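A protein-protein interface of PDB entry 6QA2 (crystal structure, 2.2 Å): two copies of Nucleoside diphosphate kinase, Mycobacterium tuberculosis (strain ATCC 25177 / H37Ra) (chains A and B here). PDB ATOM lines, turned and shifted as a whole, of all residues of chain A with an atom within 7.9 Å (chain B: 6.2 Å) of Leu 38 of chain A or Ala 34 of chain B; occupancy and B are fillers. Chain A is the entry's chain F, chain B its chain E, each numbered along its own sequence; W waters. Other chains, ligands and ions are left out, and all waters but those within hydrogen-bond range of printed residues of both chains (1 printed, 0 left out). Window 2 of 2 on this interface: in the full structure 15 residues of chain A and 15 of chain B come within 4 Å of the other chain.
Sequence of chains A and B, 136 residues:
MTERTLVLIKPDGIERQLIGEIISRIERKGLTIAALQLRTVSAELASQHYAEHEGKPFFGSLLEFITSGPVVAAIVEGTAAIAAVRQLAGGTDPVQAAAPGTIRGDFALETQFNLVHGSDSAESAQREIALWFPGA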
ATOM      1  N   ILE A   9      -4.754  10.721  -0.067  1.00  0.00           N
ATOM      2  CA  ILE A   9      -3.398  11.172   0.219  1.00  0.00           C
ATOM      3  C   ILE A   9      -2.471  10.031  -0.184  1.00  0.00           C
ATOM      4  O   ILE A   9      -2.472   8.966   0.440  1.00  0.00           O
ATOM      5  CB  ILE A   9      -3.221  11.555   1.693  1.00  0.00           C
ATOM      6  CG1 ILE A   9      -4.299  12.564   2.102  1.00  0.00           C
ATOM      7  CG2 ILE A   9      -1.827  12.132   1.923  1.00  0.00           C
ATOM      8  CD1 ILE A   9      -4.142  13.115   3.508  1.00  0.00           C
ATOM      9  N   ILE A  14       2.016  10.629   2.691  1.00  0.00           N
ATOM     10  CA  ILE A  14       2.121  10.090   4.044  1.00  0.00           C
ATOM     11  C   ILE A  14       3.578  10.040   4.483  1.00  0.00           C
ATOM     12  O   ILE A  14       3.923  10.433   5.604  1.00  0.00           O
ATOM     13  CB  ILE A  14       1.466   8.699   4.113  1.00  0.00           C
ATOM     14  CG1 ILE A  14      -0.049   8.822   3.929  1.00  0.00           C
ATOM     15  CG2 ILE A  14       1.808   8.012   5.430  1.00  0.00           C
ATOM     16  CD1 ILE A  14      -0.735   7.509   3.646  1.00  0.00           C
ATOM     17  N   ILE A  19      -0.076  14.642   6.251  1.00  0.00           N
ATOM     18  CA  ILE A  19      -1.484  14.274   6.369  1.00  0.00           C
ATOM     19  C   ILE A  19      -2.290  15.437   6.935  1.00  0.00           C
ATOM     20  O   ILE A  19      -3.298  15.858   6.356  1.00  0.00           O
ATOM     21  CB  ILE A  19      -1.640  13.009   7.231  1.00  0.00           C
ATOM     22  CG1 ILE A  19      -0.933  11.824   6.567  1.00  0.00           C
ATOM     23  CG2 ILE A  19      -3.121  12.698   7.453  1.00  0.00           C
ATOM     24  CD1 ILE A  19      -0.840  10.588   7.441  1.00  0.00           C
ATOM     25  N   LEU A  36     -12.878   9.043   6.854  1.00  0.00           N
ATOM     26  CA  LEU A  36     -11.429   9.161   6.945  1.00  0.00           C
ATOM     27  C   LEU A  36     -10.866   7.832   7.422  1.00  0.00           C
ATOM     28  O   LEU A  36     -11.371   7.263   8.392  1.00  0.00           O
ATOM     29  CB  LEU A  36     -11.040  10.289   7.907  1.00  0.00           C
ATOM     30  CG  LEU A  36      -9.555  10.619   8.037  1.00  0.00           C
ATOM     31  CD1 LEU A  36      -9.020  11.205   6.741  1.00  0.00           C
ATOM     32  CD2 LEU A  36      -9.329  11.576   9.199  1.00  0.00           C
ATOM     33  N   GLN A  37      -9.832   7.340   6.742  1.00  0.00           N
ATOM     34  CA  GLN A  37      -9.219   6.079   7.140  1.00  0.00           C
ATOM     35  C   GLN A  37      -7.854   5.942   6.486  1.00  0.00           C
ATOM     36  O   GLN A  37      -7.719   6.153   5.277  1.00  0.00           O
ATOM     37  CB  GLN A  37     -10.110   4.890   6.761  1.00  0.00           C
ATOM     38  CG  GLN A  37      -9.545   3.538   7.178  1.00  0.00           C
ATOM     39  CD  GLN A  37     -10.588   2.434   7.157  1.00  0.00           C
ATOM     40  OE1 GLN A  37     -11.787   2.698   7.062  1.00  0.00           O
ATOM     41  NE2 GLN A  37     -10.135   1.190   7.249  1.00  0.00           N
ATOM     42  N   LEU A  38      -6.851   5.593   7.289  1.00  0.00           N
ATOM     43  CA  LEU A  38      -5.547   5.211   6.766  1.00  0.00           C
ATOM     44  C   LEU A  38      -5.602   3.764   6.300  1.00  0.00           C
ATOM     45  O   LEU A  38      -6.014   2.876   7.053  1.00  0.00           O
ATOM     46  CB  LEU A  38      -4.469   5.388   7.836  1.00  0.00           C
ATOM     47  CG  LEU A  38      -3.079   4.827   7.523  1.00  0.00           C
ATOM     48  CD1 LEU A  38      -2.447   5.550   6.343  1.00  0.00           C
ATOM     49  CD2 LEU A  38      -2.186   4.917   8.749  1.00  0.00           C
ATOM     50  N   ARG A  39      -5.184   3.527   5.059  1.00  0.00           N
ATOM     51  CA  ARG A  39      -5.288   2.219   4.433  1.00  0.00           C
ATOM     52  C   ARG A  39      -3.928   1.778   3.916  1.00  0.00           C
ATOM     53  O   ARG A  39      -3.025   2.590   3.700  1.00  0.00           O
ATOM     54  CB  ARG A  39      -6.292   2.231   3.269  1.00  0.00           C
ATOM     55  CG  ARG A  39      -7.714   2.603   3.660  1.00  0.00           C
ATOM     56  CD  ARG A  39      -8.539   1.372   3.996  1.00  0.00           C
ATOM     57  NE  ARG A  39      -8.739   0.514   2.830  1.00  0.00           N
ATOM     58  CZ  ARG A  39      -9.750   0.625   1.972  1.00  0.00           C
ATOM     59  NH1 ARG A  39     -10.674   1.563   2.134  1.00  0.00           N
ATOM     60  NH2 ARG A  39      -9.837  -0.208   0.944  1.00  0.00           N
ATOM     61  N   THR A  40      -3.795   0.468   3.720  1.00  0.00           N
ATOM     62  CA  THR A  40      -2.648  -0.122   3.040  1.00  0.00           C
ATOM     63  C   THR A  40      -3.156  -0.838   1.797  1.00  0.00           C
ATOM     64  O   THR A  40      -4.009  -1.726   1.895  1.00  0.00           O
ATOM     65  CB  THR A  40      -1.894  -1.096   3.949  1.00  0.00           C
ATOM     66  OG1 THR A  40      -2.822  -2.006   4.554  1.00  0.00           O
ATOM     67  CG2 THR A  40      -1.133  -0.347   5.030  1.00  0.00           C
ATOM     68  N   VAL A  41      -2.643  -0.445   0.636  1.00  0.00           N
ATOM     69  CA  VAL A  41      -3.015  -1.049  -0.637  1.00  0.00           C
ATOM     70  C   VAL A  41      -1.828  -1.854  -1.147  1.00  0.00           C
ATOM     71  O   VAL A  41      -0.676  -1.419  -1.040  1.00  0.00           O
ATOM     72  CB  VAL A  41      -3.453   0.012  -1.666  1.00  0.00           C
ATOM     73  CG1 VAL A  41      -3.854  -0.652  -2.976  1.00  0.00           C
ATOM     74  CG2 VAL A  41      -4.603   0.838  -1.112  1.00  0.00           C
ATOM     75  N   GLY A  69       0.962   0.981  -1.581  1.00  0.00           N
ATOM     76  CA  GLY A  69       1.549   1.615  -0.427  1.00  0.00           C
ATOM     77  C   GLY A  69       0.493   2.171   0.505  1.00  0.00           C
ATOM     78  O   GLY A  69      -0.711   2.008   0.281  1.00  0.00           O
ATOM     79  N   PRO A  70       0.923   2.837   1.576  1.00  0.00           N
ATOM     80  CA  PRO A  70      -0.047   3.445   2.493  1.00  0.00           C
ATOM     81  C   PRO A  70      -0.745   4.628   1.844  1.00  0.00           C
ATOM     82  O   PRO A  70      -0.145   5.394   1.086  1.00  0.00           O
ATOM     83  CB  PRO A  70       0.814   3.881   3.683  1.00  0.00           C
ATOM     84  CG  PRO A  70       2.165   4.100   3.101  1.00  0.00           C
ATOM     85  CD  PRO A  70       2.312   3.083   1.999  1.00  0.00           C
ATOM     86  N   VAL A  71      -2.031   4.773   2.153  1.00  0.00           N
ATOM     87  CA  VAL A  71      -2.849   5.840   1.590  1.00  0.00           C
ATOM     88  C   VAL A  71      -3.929   6.193   2.601  1.00  0.00           C
ATOM     89  O   VAL A  71      -4.439   5.328   3.318  1.00  0.00           O
ATOM     90  CB  VAL A  71      -3.459   5.428   0.230  1.00  0.00           C
ATOM     91  CG1 VAL A  71      -4.051   4.030   0.315  1.00  0.00           C
ATOM     92  CG2 VAL A  71      -4.519   6.427  -0.210  1.00  0.00           C
ATOM     93  N   VAL A  72      -4.265   7.477   2.665  1.00  0.00           N
ATOM     94  CA  VAL A  72      -5.357   7.968   3.499  1.00  0.00           C
ATOM     95  C   VAL A  72      -6.511   8.327   2.578  1.00  0.00           C
ATOM     96  O   VAL A  72      -6.395   9.240   1.751  1.00  0.00           O
ATOM     97  CB  VAL A  72      -4.934   9.177   4.346  1.00  0.00           C
ATOM     98  CG1 VAL A  72      -6.153   9.824   4.989  1.00  0.00           C
ATOM     99  CG2 VAL A  72      -3.928   8.760   5.408  1.00  0.00           C
ATOM    100  N   ALA A  73      -7.618   7.605   2.712  1.00  0.00           N
ATOM    101  CA  ALA A  73      -8.834   7.891   1.970  1.00  0.00           C
ATOM    102  C   ALA A  73      -9.769   8.731   2.828  1.00  0.00           C
ATOM    103  O   ALA A  73      -9.810   8.591   4.053  1.00  0.00           O
ATOM    104  CB  ALA A  73      -9.537   6.601   1.544  1.00  0.00           C
ATOM    105  N   ALA A  74     -10.522   9.611   2.174  1.00  0.00           N
ATOM    106  CA  ALA A  74     -11.453  10.473   2.884  1.00  0.00           C
ATOM    107  C   ALA A  74     -12.583  10.882   1.956  1.00  0.00           C
ATOM    108  O   ALA A  74     -12.368  11.109   0.762  1.00  0.00           O
ATOM    109  CB  ALA A  74     -10.749  11.722   3.431  1.00  0.00           C
ATOM    110  N   TRP A 132     -13.987   2.774  -1.854  1.00  0.00           N
ATOM    111  CA  TRP A 132     -13.163   2.945  -0.664  1.00  0.00           C
ATOM    112  C   TRP A 132     -13.967   2.935   0.627  1.00  0.00           C
ATOM    113  O   TRP A 132     -13.435   2.547   1.674  1.00  0.00           O
ATOM    114  CB  TRP A 132     -12.370   4.251  -0.765  1.00  0.00           C
ATOM    115  CG  TRP A 132     -11.313   4.215  -1.828  1.00  0.00           C
ATOM    116  CD1 TRP A 132     -11.474   4.490  -3.154  1.00  0.00           C
ATOM    117  CD2 TRP A 132      -9.932   3.876  -1.654  1.00  0.00           C
ATOM    118  NE1 TRP A 132     -10.279   4.350  -3.816  1.00  0.00           N
ATOM    119  CE2 TRP A 132      -9.317   3.972  -2.917  1.00  0.00           C
ATOM    120  CE3 TRP A 132      -9.156   3.504  -0.552  1.00  0.00           C
ATOM    121  CZ2 TRP A 132      -7.964   3.709  -3.109  1.00  0.00           C
ATOM    122  CZ3 TRP A 132      -7.814   3.244  -0.745  1.00  0.00           C
ATOM    123  CH2 TRP A 132      -7.231   3.346  -2.012  1.00  0.00           C
ATOM    124  N   PHE A 133     -15.232   3.348   0.583  1.00  0.00           N
ATOM    125  CA  PHE A 133     -16.097   3.384   1.761  1.00  0.00           C
ATOM    126  C   PHE A 133     -17.406   2.690   1.413  1.00  0.00           C
ATOM    127  O   PHE A 133     -18.394   3.342   1.048  1.00  0.00           O
ATOM    128  CB  PHE A 133     -16.330   4.821   2.230  1.00  0.00           C
ATOM    129  CG  PHE A 133     -15.098   5.485   2.770  1.00  0.00           C
ATOM    130  CD1 PHE A 133     -14.689   5.257   4.074  1.00  0.00           C
ATOM    131  CD2 PHE A 133     -14.344   6.331   1.975  1.00  0.00           C
ATOM    132  CE1 PHE A 133     -13.552   5.863   4.576  1.00  0.00           C
ATOM    133  CE2 PHE A 133     -13.206   6.941   2.471  1.00  0.00           C
ATOM    134  CZ  PHE A 133     -12.811   6.707   3.773  1.00  0.00           C
ATOM    135  N   ARG B   4       3.607   2.962  21.123  1.00  0.00           N
ATOM    136  CA  ARG B   4       2.341   3.275  20.478  1.00  0.00           C
ATOM    137  C   ARG B   4       1.382   3.832  21.520  1.00  0.00           C
ATOM    138  O   ARG B   4       1.380   3.390  22.674  1.00  0.00           O
ATOM    139  CB  ARG B   4       1.717   2.042  19.820  1.00  0.00           C
ATOM    140  CG  ARG B   4       2.579   1.378  18.765  1.00  0.00           C
ATOM    141  CD  ARG B   4       1.787   0.311  18.027  1.00  0.00           C
ATOM    142  NE  ARG B   4       1.121  -0.606  18.949  1.00  0.00           N
ATOM    143  CZ  ARG B   4       0.277  -1.565  18.577  1.00  0.00           C
ATOM    144  NH1 ARG B   4      -0.014  -1.742  17.294  1.00  0.00           N
ATOM    145  NH2 ARG B   4      -0.279  -2.347  19.492  1.00  0.00           N
ATOM    146  N   THR B  32       4.551   9.369  13.946  1.00  0.00           N
ATOM    147  CA  THR B  32       3.901   8.848  12.754  1.00  0.00           C
ATOM    148  C   THR B  32       2.493   8.370  13.087  1.00  0.00           C
ATOM    149  O   THR B  32       2.205   7.958  14.215  1.00  0.00           O
ATOM    150  CB  THR B  32       4.704   7.692  12.144  1.00  0.00           C
ATOM    151  OG1 THR B  32       4.909   6.673  13.130  1.00  0.00           O
ATOM    152  CG2 THR B  32       6.051   8.186  11.636  1.00  0.00           C
ATOM    153  N   ILE B  33       1.620   8.429  12.086  1.00  0.00           N
ATOM    154  CA  ILE B  33       0.237   7.984  12.222  1.00  0.00           C
ATOM    155  C   ILE B  33       0.185   6.540  11.737  1.00  0.00           C
ATOM    156  O   ILE B  33       0.232   6.272  10.535  1.00  0.00           O
ATOM    157  CB  ILE B  33      -0.726   8.880  11.440  1.00  0.00           C
ATOM    158  CG1 ILE B  33      -0.581  10.341  11.880  1.00  0.00           C
ATOM    159  CG2 ILE B  33      -2.161   8.401  11.615  1.00  0.00           C
ATOM    160  CD1 ILE B  33      -0.911  10.593  13.341  1.00  0.00           C
ATOM    161  N   ALA B  34       0.089   5.600  12.681  1.00  0.00           N
ATOM    162  CA  ALA B  34       0.045   4.182  12.349  1.00  0.00           C
ATOM    163  C   ALA B  34      -1.365   3.695  12.050  1.00  0.00           C
ATOM    164  O   ALA B  34      -1.530   2.705  11.327  1.00  0.00           O
ATOM    165  CB  ALA B  34       0.636   3.355  13.494  1.00  0.00           C
ATOM    166  N   ALA B  35      -2.381   4.361  12.591  1.00  0.00           N
ATOM    167  CA  ALA B  35      -3.767   4.026  12.302  1.00  0.00           C
ATOM    168  C   ALA B  35      -4.601   5.289  12.441  1.00  0.00           C
ATOM    169  O   ALA B  35      -4.277   6.178  13.233  1.00  0.00           O
ATOM    170  CB  ALA B  35      -4.296   2.926  13.229  1.00  0.00           C
ATOM    171  N   LEU B  36      -5.673   5.362  11.656  1.00  0.00           N
ATOM    172  CA  LEU B  36      -6.506   6.557  11.607  1.00  0.00           C
ATOM    173  C   LEU B  36      -7.879   6.162  11.095  1.00  0.00           C
ATOM    174  O   LEU B  36      -7.981   5.435  10.103  1.00  0.00           O
ATOM    175  CB  LEU B  36      -5.879   7.621  10.696  1.00  0.00           C
ATOM    176  CG  LEU B  36      -6.614   8.959  10.593  1.00  0.00           C
ATOM    177  CD1 LEU B  36      -6.518   9.724  11.903  1.00  0.00           C
ATOM    178  CD2 LEU B  36      -6.058   9.786   9.442  1.00  0.00           C
ATOM    179  N   GLN B  37      -8.930   6.634  11.765  1.00  0.00           N
ATOM    180  CA  GLN B  37     -10.285   6.335  11.322  1.00  0.00           C
ATOM    181  C   GLN B  37     -11.268   7.302  11.962  1.00  0.00           C
ATOM    182  O   GLN B  37     -11.271   7.468  13.185  1.00  0.00           O
ATOM    183  CB  GLN B  37     -10.675   4.895  11.668  1.00  0.00           C
ATOM    184  CG  GLN B  37     -12.005   4.467  11.068  1.00  0.00           C
ATOM    185  CD  GLN B  37     -12.529   3.178  11.660  1.00  0.00           C
ATOM    186  OE1 GLN B  37     -12.210   2.827  12.797  1.00  0.00           O
ATOM    187  NE2 GLN B  37     -13.341   2.462  10.892  1.00  0.00           N
ATOM    188  N   ILE B  75      -3.748   5.686  16.135  1.00  0.00           N
ATOM    189  CA  ILE B  75      -2.563   5.165  16.803  1.00  0.00           C
ATOM    190  C   ILE B  75      -1.386   6.035  16.384  1.00  0.00           C
ATOM    191  O   ILE B  75      -1.120   6.198  15.188  1.00  0.00           O
ATOM    192  CB  ILE B  75      -2.311   3.690  16.454  1.00  0.00           C
ATOM    193  CG1 ILE B  75      -3.513   2.833  16.860  1.00  0.00           C
ATOM    194  CG2 ILE B  75      -1.045   3.188  17.148  1.00  0.00           C
ATOM    195  CD1 ILE B  75      -3.367   1.363  16.510  1.00  0.00           C
ATOM    196  N   VAL B  76      -0.691   6.601  17.364  1.00  0.00           N
ATOM    197  CA  VAL B  76       0.471   7.448  17.130  1.00  0.00           C
ATOM    198  C   VAL B  76       1.697   6.704  17.637  1.00  0.00           C
ATOM    199  O   VAL B  76       1.705   6.207  18.769  1.00  0.00           O
ATOM    200  CB  VAL B  76       0.318   8.813  17.822  1.00  0.00           C
ATOM    201  CG1 VAL B  76       1.541   9.683  17.574  1.00  0.00           C
ATOM    202  CG2 VAL B  76      -0.945   9.508  17.330  1.00  0.00           C
ATOM    203  N   GLU B  77       2.727   6.625  16.798  1.00  0.00           N
ATOM    204  CA  GLU B  77       3.881   5.780  17.065  1.00  0.00           C
ATOM    205  C   GLU B  77       5.158   6.603  16.989  1.00  0.00           C
ATOM    206  O   GLU B  77       5.236   7.593  16.256  1.00  0.00           O
ATOM    207  CB  GLU B  77       3.945   4.615  16.068  1.00  0.00           C
ATOM    208  CG  GLU B  77       4.916   3.515  16.450  1.00  0.00           C
ATOM    209  CD  GLU B  77       4.712   2.255  15.632  1.00  0.00           C
ATOM    210  OE1 GLU B  77       3.969   2.308  14.630  1.00  0.00           O
ATOM    211  OE2 GLU B  77       5.291   1.209  15.996  1.00  0.00           O
HETATM  212  O   HOH W   1      -5.985   2.948   9.777  1.00  0.00           O
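The backbone carbonyl oxygen of Leu 36 of chain B sits at hydrogen-bond distance from the backbone NH of Leu 38 of chain A, 3.0 Å away.
The backbone NH (N) of Ile 75 of chain B is in hydrogen-bond range of the backbone carbonyl oxygen (O) of Ala 35 of chain B (3.0 Å). The backbone NH of Ala 73 of chain A lies within hydrogen-bond range of the backbone carbonyl oxygen of Gln 37 of chain A (2.9 Å). N of Ala 34 of chain B is in hydrogen-bond range of O of Ile 75 of chain B, 2.8 Å away.
CD2 of Leu 36 of chain A touches CD2 of Leu 36 of chain B, 3.7 Å away. Gln 37 of chain B touches Leu 36 of chain A (CA to O, 3.3 Å). CA of Gln 37 of chain A touches O of Leu 36 of chain B, at 3.3 Å. Ile 33 of chain B touches Leu 38 of chain A. Leu 38 of chain A touches Ala 34 of chain B. Ala 35 of chain B touches Leu 38 of chain A.
Of chain B, only Ile 33, Ala 34, Ala 35 and Leu 36 come within 4 Å of Leu 38 of chain A. Printed residues of chain A within 4 Å of Ala 34 of chain B: Leu 38 (3.5 Å). Of the printed residues of chain A, Ala 35 of chain B touches Leu 38 (3.9 Å). Of the printed residues of chain A, Ile 33 of chain B touches Leu 38. Of the printed residues of chain B, Leu 36 of chain A touches Leu 36 (3.7 Å) and Gln 37 (3.3 Å). The nearest residue of chain A that does not touch Ala 34 of chain B is Thr 40 of chain A (7.0 Å).
Hydrophobic or aromatic side chains of chain B within 4 Å of the printed part of chain A: Leu 36. Hydrophobic or aromatic side chains of chain A within 4 Å of the printed part of chain B: Leu 36 and Leu 38. Among the printed residues, 7 pairs touch across the chains. Among the printed residues, no Asp or Glu carboxylate lies within 4 Å of a Lys or Arg side-chain nitrogen of the other chain.
Leu 36 of chain B touches its own counterpart, Leu 36 of chain A. Leu 36 of chain A touches Gln 37 of chain B, and with the chains exchanged Gln 37 of chain A touches Leu 36 of chain B. 2 positions are printed for both chains. Of the 7 pairs that touch across the chains among the printed residues, 3 have their exchanged pair printed and touching as well.
Water W1 bridges O of Leu 38 of chain A (2.7 Å) and N of Leu 36 of chain B (3.1 Å).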
